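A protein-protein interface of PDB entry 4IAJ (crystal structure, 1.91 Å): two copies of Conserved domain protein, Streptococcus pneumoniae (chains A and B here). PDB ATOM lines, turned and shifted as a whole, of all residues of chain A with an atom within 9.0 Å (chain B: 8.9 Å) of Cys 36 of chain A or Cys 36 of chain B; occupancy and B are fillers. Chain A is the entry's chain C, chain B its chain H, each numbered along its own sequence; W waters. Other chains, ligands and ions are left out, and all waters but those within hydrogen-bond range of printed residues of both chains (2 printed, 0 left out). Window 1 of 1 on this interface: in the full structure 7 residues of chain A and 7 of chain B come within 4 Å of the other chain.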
ATOM      1  N   PHE A  23     -15.407 -15.642  32.051  1.00  0.00           N
ATOM      2  CA  PHE A  23     -16.029 -14.347  32.170  1.00  0.00           C
ATOM      3  C   PHE A  23     -15.401 -13.582  33.342  1.00  0.00           C
ATOM      4  O   PHE A  23     -15.123 -14.150  34.411  1.00  0.00           O
ATOM      5  CB  PHE A  23     -17.538 -14.513  32.377  1.00  0.00           C
ATOM      6  CG  PHE A  23     -18.223 -15.231  31.253  1.00  0.00           C
ATOM      7  CD1 PHE A  23     -18.662 -14.542  30.144  1.00  0.00           C
ATOM      8  CD2 PHE A  23     -18.382 -16.603  31.294  1.00  0.00           C
ATOM      9  CE1 PHE A  23     -19.281 -15.204  29.096  1.00  0.00           C
ATOM     10  CE2 PHE A  23     -18.993 -17.275  30.253  1.00  0.00           C
ATOM     11  CZ  PHE A  23     -19.437 -16.574  29.144  1.00  0.00           C
ATOM     12  N   PHE A  29     -21.148 -12.559  32.148  1.00  0.00           N
ATOM     13  CA  PHE A  29     -21.874 -13.817  31.952  1.00  0.00           C
ATOM     14  C   PHE A  29     -23.377 -13.585  31.667  1.00  0.00           C
ATOM     15  O   PHE A  29     -23.928 -14.105  30.701  1.00  0.00           O
ATOM     16  CB  PHE A  29     -21.684 -14.731  33.174  1.00  0.00           C
ATOM     17  CG  PHE A  29     -22.459 -15.999  33.086  1.00  0.00           C
ATOM     18  CD1 PHE A  29     -22.121 -16.953  32.147  1.00  0.00           C
ATOM     19  CD2 PHE A  29     -23.594 -16.196  33.868  1.00  0.00           C
ATOM     20  CE1 PHE A  29     -22.859 -18.117  32.012  1.00  0.00           C
ATOM     21  CE2 PHE A  29     -24.337 -17.359  33.743  1.00  0.00           C
ATOM     22  CZ  PHE A  29     -23.964 -18.324  32.817  1.00  0.00           C
ATOM     23  N   GLU A  30     -24.041 -12.773  32.460  1.00  0.00           N
ATOM     24  CA  GLU A  30     -25.446 -12.451  32.184  1.00  0.00           C
ATOM     25  C   GLU A  30     -25.665 -11.840  30.787  1.00  0.00           C
ATOM     26  O   GLU A  30     -26.614 -12.211  30.075  1.00  0.00           O
ATOM     27  CB  GLU A  30     -25.993 -11.463  33.196  1.00  0.00           C
ATOM     28  CG  GLU A  30     -26.186 -12.005  34.585  1.00  0.00           C
ATOM     29  CD  GLU A  30     -26.927 -11.018  35.444  1.00  0.00           C
ATOM     30  OE1 GLU A  30     -26.529  -9.835  35.434  1.00  0.00           O
ATOM     31  OE2 GLU A  30     -27.910 -11.417  36.098  1.00  0.00           O
ATOM     32  N   ARG A  31     -24.819 -10.883  30.409  1.00  0.00           N
ATOM     33  CA  ARG A  31     -24.907 -10.257  29.088  1.00  0.00           C
ATOM     34  C   ARG A  31     -24.809 -11.309  27.967  1.00  0.00           C
ATOM     35  O   ARG A  31     -25.583 -11.283  26.994  1.00  0.00           O
ATOM     36  CB  ARG A  31     -23.809  -9.205  28.927  1.00  0.00           C
ATOM     37  CG  ARG A  31     -23.909  -8.368  27.666  1.00  0.00           C
ATOM     38  CD  ARG A  31     -22.873  -7.254  27.627  1.00  0.00           C
ATOM     39  NE  ARG A  31     -21.534  -7.784  27.376  1.00  0.00           N
ATOM     40  CZ  ARG A  31     -20.500  -7.616  28.191  1.00  0.00           C
ATOM     41  NH1 ARG A  31     -20.633  -6.909  29.308  1.00  0.00           N
ATOM     42  NH2 ARG A  31     -19.330  -8.152  27.879  1.00  0.00           N
ATOM     43  N   SER A  32     -23.860 -12.230  28.105  1.00  0.00           N
ATOM     44  CA  SER A  32     -23.710 -13.323  27.130  1.00  0.00           C
ATOM     45  C   SER A  32     -24.978 -14.191  27.051  1.00  0.00           C
ATOM     46  O   SER A  32     -25.340 -14.660  25.973  1.00  0.00           O
ATOM     47  CB  SER A  32     -22.469 -14.187  27.426  1.00  0.00           C
ATOM     48  OG  SER A  32     -22.734 -15.168  28.422  1.00  0.00           O
ATOM     49  N   GLN A  33     -25.678 -14.375  28.172  1.00  0.00           N
ATOM     50  CA  GLN A  33     -26.921 -15.133  28.144  1.00  0.00           C
ATOM     51  C   GLN A  33     -28.023 -14.342  27.435  1.00  0.00           C
ATOM     52  O   GLN A  33     -28.790 -14.917  26.667  1.00  0.00           O
ATOM     53  CB  GLN A  33     -27.316 -15.560  29.562  1.00  0.00           C
ATOM     54  CG  GLN A  33     -26.304 -16.515  30.187  1.00  0.00           C
ATOM     55  CD  GLN A  33     -26.450 -17.957  29.707  1.00  0.00           C
ATOM     56  OE1 GLN A  33     -27.453 -18.603  29.964  1.00  0.00           O
ATOM     57  NE2 GLN A  33     -25.438 -18.464  29.037  1.00  0.00           N
ATOM     58  N   GLN A  34     -28.081 -13.037  27.663  1.00  0.00           N
ATOM     59  CA  GLN A  34     -29.080 -12.213  27.040  1.00  0.00           C
ATOM     60  C   GLN A  34     -28.834 -12.087  25.530  1.00  0.00           C
ATOM     61  O   GLN A  34     -29.784 -11.971  24.789  1.00  0.00           O
ATOM     62  CB  GLN A  34     -29.133 -10.824  27.687  1.00  0.00           C
ATOM     63  CG  GLN A  34     -30.253  -9.945  27.135  1.00  0.00           C
ATOM     64  CD  GLN A  34     -30.523  -8.693  27.949  1.00  0.00           C
ATOM     65  OE1 GLN A  34     -29.667  -8.220  28.689  1.00  0.00           O
ATOM     66  NE2 GLN A  34     -31.730  -8.141  27.803  1.00  0.00           N
ATOM     67  N   ALA A  35     -27.576 -12.132  25.099  1.00  0.00           N
ATOM     68  CA  ALA A  35     -27.228 -11.871  23.696  1.00  0.00           C
ATOM     69  C   ALA A  35     -27.620 -12.990  22.717  1.00  0.00           C
ATOM     70  O   ALA A  35     -27.861 -12.698  21.542  1.00  0.00           O
ATOM     71  CB  ALA A  35     -25.736 -11.576  23.565  1.00  0.00           C
ATOM     72  N   CYS A  36     -27.645 -14.245  23.166  1.00  0.00           N
ATOM     73  CA  CYS A  36     -27.902 -15.395  22.264  1.00  0.00           C
ATOM     74  C   CYS A  36     -29.359 -15.810  22.322  1.00  0.00           C
ATOM     75  O   CYS A  36     -29.897 -15.985  23.402  1.00  0.00           O
ATOM     76  CB  CYS A  36     -27.040 -16.624  22.603  1.00  0.00           C
ATOM     77  SG  CYS A  36     -25.285 -16.257  22.667  1.00  0.00           S
ATOM     78  N   LEU A  37     -29.988 -15.955  21.168  1.00  0.00           N
ATOM     79  CA  LEU A  37     -31.287 -16.634  21.081  1.00  0.00           C
ATOM     80  C   LEU A  37     -31.072 -18.095  21.514  1.00  0.00           C
ATOM     81  O   LEU A  37     -31.800 -18.629  22.349  1.00  0.00           O
ATOM     82  CB  LEU A  37     -31.836 -16.549  19.668  1.00  0.00           C
ATOM     83  CG  LEU A  37     -33.256 -17.070  19.436  1.00  0.00           C
ATOM     84  CD1 LEU A  37     -34.246 -16.281  20.251  1.00  0.00           C
ATOM     85  CD2 LEU A  37     -33.577 -16.997  17.971  1.00  0.00           C
ATOM     86  N   ILE A  38     -30.025 -18.708  20.970  1.00  0.00           N
ATOM     87  CA  ILE A  38     -29.546 -20.013  21.406  1.00  0.00           C
ATOM     88  C   ILE A  38     -28.013 -19.973  21.451  1.00  0.00           C
ATOM     89  O   ILE A  38     -27.383 -19.572  20.476  1.00  0.00           O
ATOM     90  CB  ILE A  38     -29.983 -21.136  20.452  1.00  0.00           C
ATOM     91  CG1 ILE A  38     -31.515 -21.216  20.351  1.00  0.00           C
ATOM     92  CG2 ILE A  38     -29.394 -22.470  20.916  1.00  0.00           C
ATOM     93  CD1 ILE A  38     -31.994 -22.221  19.330  1.00  0.00           C
ATOM     94  N   GLY A  39     -27.424 -20.338  22.583  1.00  0.00           N
ATOM     95  CA  GLY A  39     -25.966 -20.419  22.707  1.00  0.00           C
ATOM     96  C   GLY A  39     -25.453 -21.689  22.055  1.00  0.00           C
ATOM     97  O   GLY A  39     -26.096 -22.711  22.194  1.00  0.00           O
ATOM     98  N   VAL A  40     -24.284 -21.656  21.408  1.00  0.00           N
ATOM     99  CA  VAL A  40     -23.734 -22.848  20.763  1.00  0.00           C
ATOM    100  C   VAL A  40     -23.628 -24.020  21.738  1.00  0.00           C
ATOM    101  O   VAL A  40     -23.910 -25.175  21.375  1.00  0.00           O
ATOM    102  CB  VAL A  40     -22.334 -22.614  20.163  1.00  0.00           C
ATOM    103  CG1 VAL A  40     -21.855 -23.871  19.447  1.00  0.00           C
ATOM    104  CG2 VAL A  40     -22.336 -21.445  19.209  1.00  0.00           C
ATOM    105  N   ALA A  41     -23.249 -23.711  22.986  1.00  0.00           N
ATOM    106  CA  ALA A  41     -22.894 -24.748  23.957  1.00  0.00           C
ATOM    107  C   ALA A  41     -24.032 -25.147  24.871  1.00  0.00           C
ATOM    108  O   ALA A  41     -23.835 -25.973  25.750  1.00  0.00           O
ATOM    109  CB  ALA A  41     -21.673 -24.309  24.791  1.00  0.00           C
ATOM    110  N   ASP A  42     -25.229 -24.598  24.650  1.00  0.00           N
ATOM    111  CA  ASP A  42     -26.301 -24.727  25.642  1.00  0.00           C
ATOM    112  C   ASP A  42     -26.639 -26.176  26.046  1.00  0.00           C
ATOM    113  O   ASP A  42     -27.012 -26.386  27.179  1.00  0.00           O
ATOM    114  CB  ASP A  42     -27.564 -24.038  25.156  1.00  0.00           C
ATOM    115  CG  ASP A  42     -27.478 -22.518  25.276  1.00  0.00           C
ATOM    116  OD1 ASP A  42     -26.493 -22.040  25.867  1.00  0.00           O
ATOM    117  OD2 ASP A  42     -28.399 -21.837  24.810  1.00  0.00           O
ATOM    118  N   TYR A  62     -24.579 -26.682  30.060  1.00  0.00           N
ATOM    119  CA  TYR A  62     -24.132 -25.315  29.992  1.00  0.00           C
ATOM    120  C   TYR A  62     -25.319 -24.359  30.090  1.00  0.00           C
ATOM    121  O   TYR A  62     -25.287 -23.408  30.882  1.00  0.00           O
ATOM    122  CB  TYR A  62     -23.349 -25.064  28.709  1.00  0.00           C
ATOM    123  CG  TYR A  62     -22.776 -23.653  28.634  1.00  0.00           C
ATOM    124  CD1 TYR A  62     -23.550 -22.582  28.204  1.00  0.00           C
ATOM    125  CD2 TYR A  62     -21.472 -23.403  29.013  1.00  0.00           C
ATOM    126  CE1 TYR A  62     -23.022 -21.298  28.159  1.00  0.00           C
ATOM    127  CE2 TYR A  62     -20.941 -22.148  28.966  1.00  0.00           C
ATOM    128  CZ  TYR A  62     -21.713 -21.094  28.532  1.00  0.00           C
ATOM    129  OH  TYR A  62     -21.147 -19.847  28.502  1.00  0.00           O
ATOM    130  N   PHE B  23     -18.433  -3.363  22.858  1.00  0.00           N
ATOM    131  CA  PHE B  23     -17.393  -4.361  23.038  1.00  0.00           C
ATOM    132  C   PHE B  23     -16.100  -3.622  23.278  1.00  0.00           C
ATOM    133  O   PHE B  23     -15.768  -2.679  22.554  1.00  0.00           O
ATOM    134  CB  PHE B  23     -17.318  -5.285  21.824  1.00  0.00           C
ATOM    135  CG  PHE B  23     -18.588  -6.050  21.600  1.00  0.00           C
ATOM    136  CD1 PHE B  23     -18.844  -7.207  22.323  1.00  0.00           C
ATOM    137  CD2 PHE B  23     -19.566  -5.565  20.740  1.00  0.00           C
ATOM    138  CE1 PHE B  23     -20.034  -7.895  22.156  1.00  0.00           C
ATOM    139  CE2 PHE B  23     -20.759  -6.249  20.560  1.00  0.00           C
ATOM    140  CZ  PHE B  23     -20.994  -7.415  21.269  1.00  0.00           C
ATOM    141  N   PHE B  29     -15.663  -8.894  20.664  1.00  0.00           N
ATOM    142  CA  PHE B  29     -16.716  -8.989  19.650  1.00  0.00           C
ATOM    143  C   PHE B  29     -16.682 -10.370  18.973  1.00  0.00           C
ATOM    144  O   PHE B  29     -17.733 -11.007  18.776  1.00  0.00           O
ATOM    145  CB  PHE B  29     -16.582  -7.845  18.629  1.00  0.00           C
ATOM    146  CG  PHE B  29     -17.558  -7.932  17.476  1.00  0.00           C
ATOM    147  CD1 PHE B  29     -18.917  -7.745  17.687  1.00  0.00           C
ATOM    148  CD2 PHE B  29     -17.111  -8.183  16.184  1.00  0.00           C
ATOM    149  CE1 PHE B  29     -19.820  -7.834  16.637  1.00  0.00           C
ATOM    150  CE2 PHE B  29     -18.006  -8.264  15.131  1.00  0.00           C
ATOM    151  CZ  PHE B  29     -19.360  -8.085  15.355  1.00  0.00           C
ATOM    152  N   GLU B  30     -15.485 -10.847  18.630  1.00  0.00           N
ATOM    153  CA  GLU B  30     -15.348 -12.175  18.027  1.00  0.00           C
ATOM    154  C   GLU B  30     -15.890 -13.273  18.948  1.00  0.00           C
ATOM    155  O   GLU B  30     -16.618 -14.161  18.489  1.00  0.00           O
ATOM    156  CB  GLU B  30     -13.886 -12.466  17.660  1.00  0.00           C
ATOM    157  CG  GLU B  30     -13.375 -11.653  16.480  1.00  0.00           C
ATOM    158  CD  GLU B  30     -11.970 -12.041  16.055  1.00  0.00           C
ATOM    159  OE1 GLU B  30     -11.120 -12.289  16.936  1.00  0.00           O
ATOM    160  OE2 GLU B  30     -11.723 -12.101  14.834  1.00  0.00           O
ATOM    161  N   ARG B  31     -15.566 -13.201  20.244  1.00  0.00           N
ATOM    162  CA  ARG B  31     -16.084 -14.193  21.214  1.00  0.00           C
ATOM    163  C   ARG B  31     -17.610 -14.205  21.264  1.00  0.00           C
ATOM    164  O   ARG B  31     -18.214 -15.278  21.368  1.00  0.00           O
ATOM    165  CB  ARG B  31     -15.526 -13.983  22.633  1.00  0.00           C
ATOM    166  CG  ARG B  31     -14.139 -14.574  22.852  1.00  0.00           C
ATOM    167  CD  ARG B  31     -13.702 -14.482  24.312  1.00  0.00           C
ATOM    168  NE  ARG B  31     -13.278 -13.134  24.697  1.00  0.00           N
ATOM    169  CZ  ARG B  31     -12.054 -12.629  24.514  1.00  0.00           C
ATOM    170  NH1 ARG B  31     -11.090 -13.348  23.935  1.00  0.00           N
ATOM    171  NH2 ARG B  31     -11.787 -11.385  24.909  1.00  0.00           N
ATOM    172  N   SER B  32     -18.231 -13.026  21.172  1.00  0.00           N
ATOM    173  CA  SER B  32     -19.691 -12.936  21.161  1.00  0.00           C
ATOM    174  C   SER B  32     -20.280 -13.591  19.910  1.00  0.00           C
ATOM    175  O   SER B  32     -21.364 -14.177  19.958  1.00  0.00           O
ATOM    176  CB  SER B  32     -20.151 -11.476  21.269  1.00  0.00           C
ATOM    177  OG  SER B  32     -19.911 -10.758  20.058  1.00  0.00           O
ATOM    178  N   GLN B  33     -19.588 -13.481  18.778  1.00  0.00           N
ATOM    179  CA  GLN B  33     -20.085 -14.075  17.545  1.00  0.00           C
ATOM    180  C   GLN B  33     -19.980 -15.598  17.604  1.00  0.00           C
ATOM    181  O   GLN B  33     -20.900 -16.301  17.187  1.00  0.00           O
ATOM    182  CB  GLN B  33     -19.347 -13.482  16.346  1.00  0.00           C
ATOM    183  CG  GLN B  33     -19.777 -12.045  16.078  1.00  0.00           C
ATOM    184  CD  GLN B  33     -21.198 -11.972  15.547  1.00  0.00           C
ATOM    185  OE1 GLN B  33     -21.615 -12.834  14.784  1.00  0.00           O
ATOM    186  NE2 GLN B  33     -21.944 -10.967  15.959  1.00  0.00           N
ATOM    187  N   GLN B  34     -18.875 -16.094  18.146  1.00  0.00           N
ATOM    188  CA  GLN B  34     -18.651 -17.523  18.253  1.00  0.00           C
ATOM    189  C   GLN B  34     -19.581 -18.176  19.290  1.00  0.00           C
ATOM    190  O   GLN B  34     -19.929 -19.345  19.135  1.00  0.00           O
ATOM    191  CB  GLN B  34     -17.190 -17.819  18.615  1.00  0.00           C
ATOM    192  CG  GLN B  34     -16.892 -19.312  18.675  1.00  0.00           C
ATOM    193  CD  GLN B  34     -15.431 -19.666  18.427  1.00  0.00           C
ATOM    194  OE1 GLN B  34     -14.518 -18.942  18.834  1.00  0.00           O
ATOM    195  NE2 GLN B  34     -15.206 -20.798  17.758  1.00  0.00           N
ATOM    196  N   ALA B  35     -19.988 -17.422  20.310  1.00  0.00           N
ATOM    197  CA  ALA B  35     -20.777 -17.974  21.423  1.00  0.00           C
ATOM    198  C   ALA B  35     -22.230 -18.284  21.083  1.00  0.00           C
ATOM    199  O   ALA B  35     -22.814 -19.172  21.706  1.00  0.00           O
ATOM    200  CB  ALA B  35     -20.735 -17.034  22.624  1.00  0.00           C
ATOM    201  N   CYS B  36     -22.847 -17.529  20.168  1.00  0.00           N
ATOM    202  CA  CYS B  36     -24.216 -17.750  19.814  1.00  0.00           C
ATOM    203  C   CYS B  36     -24.350 -18.603  18.575  1.00  0.00           C
ATOM    204  O   CYS B  36     -23.699 -18.361  17.567  1.00  0.00           O
ATOM    205  CB  CYS B  36     -24.991 -16.437  19.576  1.00  0.00           C
ATOM    206  SG  CYS B  36     -24.890 -15.249  20.918  1.00  0.00           S
ATOM    207  N   LEU B  37     -25.212 -19.608  18.662  1.00  0.00           N
ATOM    208  CA  LEU B  37     -25.677 -20.294  17.472  1.00  0.00           C
ATOM    209  C   LEU B  37     -26.470 -19.298  16.612  1.00  0.00           C
ATOM    210  O   LEU B  37     -26.235 -19.165  15.403  1.00  0.00           O
ATOM    211  CB  LEU B  37     -26.529 -21.495  17.865  1.00  0.00           C
ATOM    212  CG  LEU B  37     -26.952 -22.404  16.706  1.00  0.00           C
ATOM    213  CD1 LEU B  37     -25.732 -22.941  15.992  1.00  0.00           C
ATOM    214  CD2 LEU B  37     -27.859 -23.508  17.225  1.00  0.00           C
ATOM    215  N   ILE B  38     -27.380 -18.594  17.259  1.00  0.00           N
ATOM    216  CA  ILE B  38     -28.109 -17.476  16.675  1.00  0.00           C
ATOM    217  C   ILE B  38     -28.169 -16.366  17.722  1.00  0.00           C
ATOM    218  O   ILE B  38     -28.561 -16.606  18.868  1.00  0.00           O
ATOM    219  CB  ILE B  38     -29.563 -17.838  16.264  1.00  0.00           C
ATOM    220  CG1 ILE B  38     -29.598 -18.980  15.250  1.00  0.00           C
ATOM    221  CG2 ILE B  38     -30.270 -16.629  15.660  1.00  0.00           C
ATOM    222  CD1 ILE B  38     -30.982 -19.533  15.013  1.00  0.00           C
ATOM    223  N   GLY B  39     -27.754 -15.160  17.340  1.00  0.00           N
ATOM    224  CA  GLY B  39     -27.887 -13.992  18.205  1.00  0.00           C
ATOM    225  C   GLY B  39     -29.306 -13.442  18.203  1.00  0.00           C
ATOM    226  O   GLY B  39     -29.978 -13.444  17.162  1.00  0.00           O
ATOM    227  N   VAL B  40     -29.766 -12.954  19.352  1.00  0.00           N
ATOM    228  CA  VAL B  40     -31.109 -12.377  19.486  1.00  0.00           C
ATOM    229  C   VAL B  40     -31.324 -11.286  18.432  1.00  0.00           C
ATOM    230  O   VAL B  40     -32.369 -11.212  17.808  1.00  0.00           O
ATOM    231  CB  VAL B  40     -31.340 -11.813  20.906  1.00  0.00           C
ATOM    232  CG1 VAL B  40     -32.686 -11.094  21.036  1.00  0.00           C
ATOM    233  CG2 VAL B  40     -31.260 -12.927  21.941  1.00  0.00           C
ATOM    234  N   ALA B  41     -30.296 -10.474  18.231  1.00  0.00           N
ATOM    235  CA  ALA B  41     -30.378  -9.255  17.387  1.00  0.00           C
ATOM    236  C   ALA B  41     -29.959  -9.435  15.918  1.00  0.00           C
ATOM    237  O   ALA B  41     -29.958  -8.454  15.173  1.00  0.00           O
ATOM    238  CB  ALA B  41     -29.521  -8.170  18.002  1.00  0.00           C
ATOM    239  N   ASP B  42     -29.653 -10.663  15.486  1.00  0.00           N
ATOM    240  CA  ASP B  42     -29.004 -10.887  14.185  1.00  0.00           C
ATOM    241  C   ASP B  42     -29.745 -10.313  12.982  1.00  0.00           C
ATOM    242  O   ASP B  42     -29.100  -9.907  12.032  1.00  0.00           O
ATOM    243  CB  ASP B  42     -28.764 -12.382  13.935  1.00  0.00           C
ATOM    244  CG  ASP B  42     -27.574 -12.943  14.747  1.00  0.00           C
ATOM    245  OD1 ASP B  42     -26.957 -12.197  15.515  1.00  0.00           O
ATOM    246  OD2 ASP B  42     -27.298 -14.151  14.621  1.00  0.00           O
ATOM    247  N   TYR B  62     -27.489  -6.529  12.059  1.00  0.00           N
ATOM    248  CA  TYR B  62     -26.532  -6.802  13.121  1.00  0.00           C
ATOM    249  C   TYR B  62     -25.672  -8.036  12.792  1.00  0.00           C
ATOM    250  O   TYR B  62     -24.442  -8.018  12.950  1.00  0.00           O
ATOM    251  CB  TYR B  62     -27.268  -7.011  14.452  1.00  0.00           C
ATOM    252  CG  TYR B  62     -26.342  -7.236  15.630  1.00  0.00           C
ATOM    253  CD1 TYR B  62     -25.770  -8.484  15.863  1.00  0.00           C
ATOM    254  CD2 TYR B  62     -26.018  -6.204  16.497  1.00  0.00           C
ATOM    255  CE1 TYR B  62     -24.906  -8.689  16.924  1.00  0.00           C
ATOM    256  CE2 TYR B  62     -25.179  -6.407  17.568  1.00  0.00           C
ATOM    257  CZ  TYR B  62     -24.613  -7.645  17.775  1.00  0.00           C
ATOM    258  OH  TYR B  62     -23.762  -7.834  18.823  1.00  0.00           O
HETATM  259  O   HOH W   1     -27.739 -10.414  19.895  1.00  0.00           O
HETATM  260  O   HOH W   2     -22.240 -21.162  23.645  1.00  0.00           O
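The backbone NH (N) of Ile 38 of chain A lies within hydrogen-bond range of the backbone carbonyl oxygen (O) of Ile 38 of chain B.
The backbone carbonyl oxygen (O) of Ala 35 of chain A lies within hydrogen-bond range of the backbone NH (N) of Val 40 of chain B, 2.9 Å away.
The backbone carbonyl oxygen (O) of Ile 38 of chain B is in hydrogen-bond range of the backbone NH (N) of Leu 37 of chain A (2.8 Å).
The backbone carbonyl oxygen (O) of Ile 38 of chain A sits at hydrogen-bond distance from the backbone NH (N) of Leu 37 of chain B, at 2.8 Å.
O of Ala 35 of chain B lies within hydrogen-bond range of N of Val 40 of chain A, 2.9 Å away.
The side-chain sulfur (SG) of Cys 36 of chain A is disulfide-bonded to the side-chain sulfur (SG) of Cys 36 of chain B (2.1 Å).
The side-chain carboxylate (OD2) of Asp 42 of chain B lies within hydrogen-bond range of the backbone NH (N) of Gly 39 of chain B, 2.9 Å away.
N of Gly 39 of chain A sits at hydrogen-bond distance from OD2 of Asp 42 of chain A, 2.9 Å away.
SG of Cys 36 of chain B touches O of Ala 35 of chain A (3.97 Å).
Ala 35 of chain A touches Gly 39 of chain B.
Ile 38 of chain B touches Cys 36 of chain A (O to C, 3.6 Å).
C of Cys 36 of chain A touches CG2 of Val 40 of chain B (3.5 Å).
C of Gly 39 of chain B touches N of Leu 37 of chain A, 3.9 Å away.
Leu 37 of chain A touches Val 40 of chain B.
C of Cys 36 of chain B touches O of Ile 38 of chain A, at 3.7 Å.
Gln 34 of chain B touches Val 40 of chain A.
Val 40 of chain A touches Cys 36 of chain B (CG2 to C, 3.5 Å).
CG2 of Val 40 of chain A touches N of Leu 37 of chain B, at 3.5 Å.
Glu 30 of chain A touches none of the printed residues of chain B.
Printed residues of chain B within 4 Å of Ala 35 of chain A: Cys 36, Gly 39 and Val 40.
Of the printed residues of chain B, Cys 36 of chain A touches Ala 35 (3.9 Å), Cys 36 (2.1 Å), Ile 38 (3.6 Å) and Val 40 (3.5 Å).
Printed residues of chain B within 4 Å of Gly 39 of chain A: Ala 35 and Leu 37.
Of the printed residues of chain A, Cys 36 of chain B touches Ala 35 (3.97 Å), Cys 36 (2.1 Å), Ile 38 (3.7 Å) and Val 40 (3.5 Å).
Of the printed residues of chain A, Leu 37 of chain B touches Ile 38, Gly 39 and Val 40.
Of the printed residues of chain A, Ile 38 of chain B touches Cys 36, Leu 37 and Ile 38.
The nearest printed residue of chain B that does not touch Cys 36 of chain A is Gly 39 of chain B (4.3 Å).
The nearest printed residue of chain A that does not touch Cys 36 of chain B is Gly 39 of chain A (4.3 Å).
The nearest printed residue of chain A that does not touch Val 40 of chain B is Gln 33 of chain A (5.7 Å).
Printed residues of chain A that touch a printed residue of chain B: Gln 34, Ala 35, Cys 36, Leu 37, Ile 38, Gly 39 and Val 40.
Among the printed residues, 20 pairs touch across the chains.
Among the printed residues, no Asp or Glu carboxylate lies within 4 Å of a Lys or Arg side-chain nitrogen of the other chain.
Ala 35 of chain A touches Gly 39 of chain B, and with the chains exchanged Gly 39 of chain A touches Ala 35 of chain B.
Ala 35 of chain A touches Val 40 of chain B, and with the chains exchanged Val 40 of chain A touches Ala 35 of chain B.
Leu 37 of chain A touches Gly 39 of chain B, and with the chains exchanged Gly 39 of chain A touches Leu 37 of chain B.
Ile 38 of chain A touches its own counterpart, Ile 38 of chain B.
Of the 20 pairs that touch across the chains among the printed residues, 20 have their exchanged pair printed and touching as well.
Water W1 lies within hydrogen-bond range of the backbone carbonyl oxygen of Ala 35 of chain A (2.8 Å), the backbone NH of Ala 41 of chain B (3.1 Å) and the backbone NH of Val 40 of chain B (3.3 Å).
Water W2 lies within hydrogen-bond range of N of Ala 41 of chain A (2.8 Å), O of Ala 35 of chain B (2.8 Å) and N of Val 40 of chain A (3.1 Å).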
